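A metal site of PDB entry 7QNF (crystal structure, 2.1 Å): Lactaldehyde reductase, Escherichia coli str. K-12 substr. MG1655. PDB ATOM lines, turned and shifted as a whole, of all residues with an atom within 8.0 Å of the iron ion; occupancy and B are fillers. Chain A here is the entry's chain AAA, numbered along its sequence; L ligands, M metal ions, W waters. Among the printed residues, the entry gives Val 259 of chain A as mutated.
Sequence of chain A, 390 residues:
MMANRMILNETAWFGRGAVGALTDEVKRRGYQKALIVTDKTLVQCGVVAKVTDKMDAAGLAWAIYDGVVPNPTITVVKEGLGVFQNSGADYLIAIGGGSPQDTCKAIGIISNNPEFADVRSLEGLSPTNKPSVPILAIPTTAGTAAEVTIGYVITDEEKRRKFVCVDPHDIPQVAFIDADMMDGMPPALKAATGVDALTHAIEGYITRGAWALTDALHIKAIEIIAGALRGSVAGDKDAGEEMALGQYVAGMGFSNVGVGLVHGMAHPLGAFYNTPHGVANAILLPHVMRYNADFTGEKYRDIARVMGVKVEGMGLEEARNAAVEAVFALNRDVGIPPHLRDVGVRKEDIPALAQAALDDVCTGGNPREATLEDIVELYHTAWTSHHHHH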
ATOM      1  N   GLY A 143      17.831  -5.849 -33.463  1.00  0.00           N
ATOM      2  CA  GLY A 143      18.248  -6.590 -32.273  1.00  0.00           C
ATOM      3  C   GLY A 143      19.671  -6.300 -31.884  1.00  0.00           C
ATOM      4  O   GLY A 143      19.884  -5.254 -31.278  1.00  0.00           O
ATOM      5  N   THR A 144      20.603  -7.213 -32.202  1.00  0.00           N
ATOM      6  CA  THR A 144      21.844  -7.412 -31.406  1.00  0.00           C
ATOM      7  C   THR A 144      22.969  -6.454 -31.820  1.00  0.00           C
ATOM      8  O   THR A 144      23.886  -6.254 -30.991  1.00  0.00           O
ATOM      9  CB  THR A 144      22.341  -8.875 -31.461  1.00  0.00           C
ATOM     10  OG1 THR A 144      22.931  -9.120 -32.731  1.00  0.00           O
ATOM     11  CG2 THR A 144      21.243  -9.867 -31.120  1.00  0.00           C
ATOM     12  N   ALA A 145      22.944  -5.933 -33.052  1.00  0.00           N
ATOM     13  CA  ALA A 145      23.992  -5.064 -33.637  1.00  0.00           C
ATOM     14  C   ALA A 145      25.319  -5.821 -33.794  1.00  0.00           C
ATOM     15  O   ALA A 145      26.358  -5.166 -33.870  1.00  0.00           O
ATOM     16  CB  ALA A 145      24.195  -3.817 -32.805  1.00  0.00           C
ATOM     17  N   VAL A 153      28.900 -13.832 -28.041  1.00  0.00           N
ATOM     18  CA  VAL A 153      28.493 -14.658 -26.856  1.00  0.00           C
ATOM     19  C   VAL A 153      28.252 -16.110 -27.303  1.00  0.00           C
ATOM     20  O   VAL A 153      27.377 -16.382 -28.168  1.00  0.00           O
ATOM     21  CB  VAL A 153      27.265 -14.057 -26.143  1.00  0.00           C
ATOM     22  CG1 VAL A 153      27.018 -14.718 -24.796  1.00  0.00           C
ATOM     23  CG2 VAL A 153      27.406 -12.559 -25.965  1.00  0.00           C
ATOM     24  N   THR A 193      13.779  -8.665 -29.902  1.00  0.00           N
ATOM     25  CA  THR A 193      15.062  -8.113 -30.424  1.00  0.00           C
ATOM     26  C   THR A 193      15.054  -6.586 -30.270  1.00  0.00           C
ATOM     27  O   THR A 193      16.118  -6.020 -29.962  1.00  0.00           O
ATOM     28  CB  THR A 193      15.356  -8.634 -31.833  1.00  0.00           C
ATOM     29  OG1 THR A 193      14.394  -8.139 -32.758  1.00  0.00           O
ATOM     30  CG2 THR A 193      15.420 -10.150 -31.854  1.00  0.00           C
ATOM     31  N   VAL A 195      13.622  -4.845 -27.775  1.00  0.00           N
ATOM     32  CA  VAL A 195      13.892  -4.479 -26.359  1.00  0.00           C
ATOM     33  C   VAL A 195      15.337  -4.863 -25.999  1.00  0.00           C
ATOM     34  O   VAL A 195      15.939  -4.165 -25.165  1.00  0.00           O
ATOM     35  CB  VAL A 195      12.849  -5.067 -25.395  1.00  0.00           C
ATOM     36  CG1 VAL A 195      13.187  -4.727 -23.952  1.00  0.00           C
ATOM     37  CG2 VAL A 195      11.432  -4.586 -25.755  1.00  0.00           C
ATOM     38  N   ASP A 196      15.909  -5.869 -26.638  1.00  0.00           N
ATOM     39  CA  ASP A 196      17.363  -6.123 -26.571  1.00  0.00           C
ATOM     40  C   ASP A 196      18.096  -4.860 -27.029  1.00  0.00           C
ATOM     41  O   ASP A 196      19.011  -4.418 -26.300  1.00  0.00           O
ATOM     42  CB  ASP A 196      17.770  -7.379 -27.357  1.00  0.00           C
ATOM     43  CG  ASP A 196      19.250  -7.724 -27.279  1.00  0.00           C
ATOM     44  OD1 ASP A 196      19.894  -7.466 -26.209  1.00  0.00           O
ATOM     45  OD2 ASP A 196      19.759  -8.273 -28.296  1.00  0.00           O
ATOM     46  N   ALA A 197      17.724  -4.268 -28.174  1.00  0.00           N
ATOM     47  CA  ALA A 197      18.369  -3.052 -28.707  1.00  0.00           C
ATOM     48  C   ALA A 197      18.191  -1.887 -27.719  1.00  0.00           C
ATOM     49  O   ALA A 197      19.170  -1.198 -27.430  1.00  0.00           O
ATOM     50  CB  ALA A 197      17.805  -2.714 -30.065  1.00  0.00           C
ATOM     51  N   THR A 199      17.780  -2.079 -24.541  1.00  0.00           N
ATOM     52  CA  THR A 199      18.610  -2.460 -23.368  1.00  0.00           C
ATOM     53  C   THR A 199      20.069  -2.082 -23.651  1.00  0.00           C
ATOM     54  O   THR A 199      20.664  -1.396 -22.817  1.00  0.00           O
ATOM     55  CB  THR A 199      18.393  -3.929 -22.990  1.00  0.00           C
ATOM     56  OG1 THR A 199      17.024  -4.128 -22.626  1.00  0.00           O
ATOM     57  CG2 THR A 199      19.294  -4.374 -21.854  1.00  0.00           C
ATOM     58  N   HIS A 200      20.606  -2.453 -24.814  1.00  0.00           N
ATOM     59  CA  HIS A 200      21.957  -2.019 -25.244  1.00  0.00           C
ATOM     60  C   HIS A 200      22.102  -0.500 -25.086  1.00  0.00           C
ATOM     61  O   HIS A 200      23.105  -0.056 -24.541  1.00  0.00           O
ATOM     62  CB  HIS A 200      22.255  -2.432 -26.671  1.00  0.00           C
ATOM     63  CG  HIS A 200      22.363  -3.900 -26.865  1.00  0.00           C
ATOM     64  ND1 HIS A 200      22.090  -4.509 -28.068  1.00  0.00           N
ATOM     65  CD2 HIS A 200      22.665  -4.894 -26.002  1.00  0.00           C
ATOM     66  CE1 HIS A 200      22.235  -5.812 -27.950  1.00  0.00           C
ATOM     67  NE2 HIS A 200      22.597  -6.083 -26.684  1.00  0.00           N
ATOM     68  N   GLU A 203      21.573   0.674 -21.208  1.00  0.00           N
ATOM     69  CA  GLU A 203      22.732   0.213 -20.415  1.00  0.00           C
ATOM     70  C   GLU A 203      23.969   1.018 -20.851  1.00  0.00           C
ATOM     71  O   GLU A 203      24.697   1.541 -19.972  1.00  0.00           O
ATOM     72  CB  GLU A 203      22.928  -1.297 -20.537  1.00  0.00           C
ATOM     73  CG  GLU A 203      21.896  -2.117 -19.788  1.00  0.00           C
ATOM     74  CD  GLU A 203      22.439  -3.401 -19.174  1.00  0.00           C
ATOM     75  OE1 GLU A 203      22.610  -3.415 -17.925  1.00  0.00           O
ATOM     76  OE2 GLU A 203      22.686  -4.374 -19.931  1.00  0.00           O
ATOM     77  N   PHE A 254      27.644   0.734 -27.469  1.00  0.00           N
ATOM     78  CA  PHE A 254      27.794  -0.148 -26.278  1.00  0.00           C
ATOM     79  C   PHE A 254      29.003  -1.054 -26.474  1.00  0.00           C
ATOM     80  O   PHE A 254      29.718  -1.284 -25.509  1.00  0.00           O
ATOM     81  CB  PHE A 254      26.485  -0.873 -25.961  1.00  0.00           C
ATOM     82  CG  PHE A 254      26.242  -2.144 -26.738  1.00  0.00           C
ATOM     83  CD1 PHE A 254      26.838  -3.331 -26.347  1.00  0.00           C
ATOM     84  CD2 PHE A 254      25.411  -2.148 -27.841  1.00  0.00           C
ATOM     85  CE1 PHE A 254      26.601  -4.505 -27.056  1.00  0.00           C
ATOM     86  CE2 PHE A 254      25.171  -3.312 -28.541  1.00  0.00           C
ATOM     87  CZ  PHE A 254      25.758  -4.495 -28.146  1.00  0.00           C
ATOM     88  N   VAL A 259      27.902  -2.344 -21.164  1.00  0.00           N
ATOM     89  CA  VAL A 259      26.456  -2.342 -20.783  1.00  0.00           C
ATOM     90  C   VAL A 259      26.424  -2.491 -19.247  1.00  0.00           C
ATOM     91  O   VAL A 259      27.116  -1.680 -18.556  1.00  0.00           O
ATOM     92  CB  VAL A 259      25.655  -3.390 -21.585  1.00  0.00           C
ATOM     93  CG1 VAL A 259      25.403  -2.914 -23.011  1.00  0.00           C
ATOM     94  CG2 VAL A 259      26.291  -4.773 -21.637  1.00  0.00           C
ATOM     95  N   HIS A 263      22.166  -7.331 -18.868  1.00  0.00           N
ATOM     96  CA  HIS A 263      22.922  -8.322 -19.675  1.00  0.00           C
ATOM     97  C   HIS A 263      23.608  -9.345 -18.765  1.00  0.00           C
ATOM     98  O   HIS A 263      23.577 -10.549 -19.103  1.00  0.00           O
ATOM     99  CB  HIS A 263      23.893  -7.616 -20.649  1.00  0.00           C
ATOM    100  CG  HIS A 263      23.238  -7.308 -21.952  1.00  0.00           C
ATOM    101  ND1 HIS A 263      22.241  -6.360 -22.050  1.00  0.00           N
ATOM    102  CD2 HIS A 263      23.391  -7.859 -23.185  1.00  0.00           C
ATOM    103  CE1 HIS A 263      21.805  -6.329 -23.295  1.00  0.00           C
ATOM    104  NE2 HIS A 263      22.483  -7.236 -24.017  1.00  0.00           N
ATOM    105  N   ALA A 266      20.777 -11.531 -17.703  1.00  0.00           N
ATOM    106  CA  ALA A 266      20.100 -12.175 -18.850  1.00  0.00           C
ATOM    107  C   ALA A 266      20.871 -13.432 -19.266  1.00  0.00           C
ATOM    108  O   ALA A 266      20.226 -14.454 -19.592  1.00  0.00           O
ATOM    109  CB  ALA A 266      19.968 -11.204 -19.992  1.00  0.00           C
ATOM    110  N   HIS A 267      22.201 -13.376 -19.239  1.00  0.00           N
ATOM    111  CA  HIS A 267      23.089 -14.415 -19.817  1.00  0.00           C
ATOM    112  C   HIS A 267      22.899 -15.753 -19.106  1.00  0.00           C
ATOM    113  O   HIS A 267      22.749 -16.771 -19.773  1.00  0.00           O
ATOM    114  CB  HIS A 267      24.560 -13.949 -19.841  1.00  0.00           C
ATOM    115  CG  HIS A 267      24.836 -13.004 -20.973  1.00  0.00           C
ATOM    116  ND1 HIS A 267      25.966 -12.197 -21.024  1.00  0.00           N
ATOM    117  CD2 HIS A 267      24.099 -12.723 -22.074  1.00  0.00           C
ATOM    118  CE1 HIS A 267      25.922 -11.475 -22.117  1.00  0.00           C
ATOM    119  NE2 HIS A 267      24.776 -11.771 -22.780  1.00  0.00           N
ATOM    120  N   HIS A 277      17.285 -14.120 -25.495  1.00  0.00           N
ATOM    121  CA  HIS A 277      18.121 -13.082 -24.840  1.00  0.00           C
ATOM    122  C   HIS A 277      17.333 -11.772 -24.643  1.00  0.00           C
ATOM    123  O   HIS A 277      17.476 -11.128 -23.582  1.00  0.00           O
ATOM    124  CB  HIS A 277      19.405 -12.954 -25.684  1.00  0.00           C
ATOM    125  CG  HIS A 277      20.230 -11.769 -25.367  1.00  0.00           C
ATOM    126  ND1 HIS A 277      21.034 -11.703 -24.264  1.00  0.00           N
ATOM    127  CD2 HIS A 277      20.370 -10.602 -26.029  1.00  0.00           C
ATOM    128  CE1 HIS A 277      21.636 -10.538 -24.229  1.00  0.00           C
ATOM    129  NE2 HIS A 277      21.257  -9.843 -25.316  1.00  0.00           N
ATOM    130  N   GLY A 278      16.539 -11.384 -25.633  1.00  0.00           N
ATOM    131  CA  GLY A 278      15.752 -10.131 -25.607  1.00  0.00           C
ATOM    132  C   GLY A 278      14.583 -10.217 -24.645  1.00  0.00           C
ATOM    133  O   GLY A 278      14.275  -9.204 -24.013  1.00  0.00           O
ATOM    134  N   ASN A 281      16.206  -9.890 -21.178  1.00  0.00           N
ATOM    135  CA  ASN A 281      16.606  -8.477 -20.986  1.00  0.00           C
ATOM    136  C   ASN A 281      15.380  -7.643 -20.666  1.00  0.00           C
ATOM    137  O   ASN A 281      15.449  -6.816 -19.718  1.00  0.00           O
ATOM    138  CB  ASN A 281      17.252  -7.857 -22.224  1.00  0.00           C
ATOM    139  CG  ASN A 281      18.687  -8.274 -22.422  1.00  0.00           C
ATOM    140  OD1 ASN A 281      19.390  -8.602 -21.472  1.00  0.00           O
ATOM    141  ND2 ASN A 281      19.140  -8.232 -23.671  1.00  0.00           N
ATOM    142  N   CYS A 362      29.735  -8.523 -18.441  1.00  0.00           N
ATOM    143  CA  CYS A 362      28.876  -7.335 -18.675  1.00  0.00           C
ATOM    144  C   CYS A 362      28.604  -6.591 -17.368  1.00  0.00           C
ATOM    145  O   CYS A 362      28.431  -5.374 -17.434  1.00  0.00           O
ATOM    146  CB  CYS A 362      27.560  -7.734 -19.325  1.00  0.00           C
ATOM    147  SG  CYS A 362      27.769  -8.371 -21.018  1.00  0.00           S
HETATM  148  N1  LIG L   1      12.471 -13.969 -39.815  1.00  0.00           N
HETATM  149  C1  LIG L   1      12.091 -15.015 -39.072  1.00  0.00           C
HETATM  150  N2  LIG L   1      12.750 -15.630 -38.087  1.00  0.00           N
HETATM  151  C2  LIG L   1      13.947 -15.050 -37.886  1.00  0.00           C
HETATM  152  C3  LIG L   1      14.468 -13.969 -38.558  1.00  0.00           C
HETATM  153  C4  LIG L   1      13.684 -13.404 -39.584  1.00  0.00           C
HETATM  154  N3  LIG L   1      14.055 -12.359 -40.317  1.00  0.00           N
HETATM  155  N4  LIG L   1      15.725 -13.667 -38.056  1.00  0.00           N
HETATM  156  C5  LIG L   1      15.943 -14.558 -37.118  1.00  0.00           C
HETATM  157  N5  LIG L   1      14.891 -15.408 -36.955  1.00  0.00           N
HETATM  158  C6  LIG L   1      14.790 -16.517 -36.015  1.00  0.00           C
HETATM  159  C7  LIG L   1      16.006 -17.431 -36.020  1.00  0.00           C
HETATM  160  O1  LIG L   1      15.944 -18.394 -37.044  1.00  0.00           O
HETATM  161  C8  LIG L   1      15.869 -18.084 -34.647  1.00  0.00           C
HETATM  162  O2  LIG L   1      15.022 -19.223 -34.766  1.00  0.00           O
HETATM  163  O3  LIG L   1      14.712 -16.008 -34.713  1.00  0.00           O
HETATM  164  C9  LIG L   1      15.263 -16.968 -33.776  1.00  0.00           C
HETATM  165  C10 LIG L   1      16.230 -16.271 -32.857  1.00  0.00           C
HETATM  166  O4  LIG L   1      17.437 -15.961 -33.590  1.00  0.00           O
HETATM  167  P1  LIG L   1      18.755 -15.461 -32.824  1.00  0.00           P
HETATM  168  O5  LIG L   1      19.851 -15.260 -33.825  1.00  0.00           O
HETATM  169  O6  LIG L   1      19.015 -16.362 -31.663  1.00  0.00           O
HETATM  170  O7  LIG L   1      18.252 -14.041 -32.274  1.00  0.00           O
HETATM  171  P2  LIG L   1      18.940 -12.660 -31.840  1.00  0.00           P
HETATM  172  O8  LIG L   1      19.147 -11.812 -33.050  1.00  0.00           O
HETATM  173  O9  LIG L   1      18.160 -12.070 -30.711  1.00  0.00           O
HETATM  174  O10 LIG L   1      20.358 -13.180 -31.292  1.00  0.00           O
HETATM  175  C11 LIG L   1      20.473 -13.612 -29.914  1.00  0.00           C
HETATM  176  O11 LIG L   1      22.763 -12.854 -29.828  1.00  0.00           O
HETATM  177  O12 LIG L   1      23.678 -11.222 -28.471  1.00  0.00           O
HETATM  178  C12 LIG L   1      23.517 -12.582 -28.643  1.00  0.00           C
HETATM  179  O13 LIG L   1      23.383 -13.472 -26.313  1.00  0.00           O
HETATM  180  C13 LIG L   1      22.691 -13.195 -27.511  1.00  0.00           C
HETATM  181  O14 LIG L   1      23.090 -15.545 -28.123  1.00  0.00           O
HETATM  182  C14 LIG L   1      22.172 -14.467 -28.164  1.00  0.00           C
HETATM  183  C15 LIG L   1      21.910 -13.995 -29.610  1.00  0.00           C
HETATM  184 FE    FE M   1      22.140  -7.977 -25.987  1.00  0.00          FE
HETATM  185  O   HOH W   1      24.301  -8.693 -26.111  1.00  0.00           O
HETATM  186  O   HOH W   2      22.296  -8.935 -27.810  1.00  0.00           O
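The backbone carbonyl oxygen (O) of His 263 lies close to a ring nitrogen (ND1) of His 267. A ring nitrogen (ND1) of His 263 sits at hydrogen-bond distance from the side-chain carboxylate (OE2) of Glu 203 (2.9 Å). The side-chain amide nitrogen (ND2) of Asn 281 sits close to the backbone carbonyl oxygen (O) of His 277 (3.3 Å). ND2 of Asn 281 sits close to OD1 of Asp 196 (2.8 Å).
Merely in contact with the iron ion: Asn 281 (3.8 Å). Five residues have an atom within 4 Å of the iron ion: Asp 196, His 200, His 263, His 277 and Asn 281. Along chain A the residues within 4 Å of the iron ion span positions 196 to 281.
Water W2 lies within hydrogen-bond range of the side-chain carboxylate of Asp 196 (2.7 Å) and an oxygen (O12) of the ligand (2.8 Å).
The iron ion is bound by water W2 (2.1 Å), a ring nitrogen (NE2) of His 200 (2.1 Å), a ring nitrogen (NE2) of His 263 (2.1 Å), a ring nitrogen (NE2) of His 277 (2.2 Å), water W1 (2.3 Å) and the side-chain carboxylate of Asp 196 (2.3 Å).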
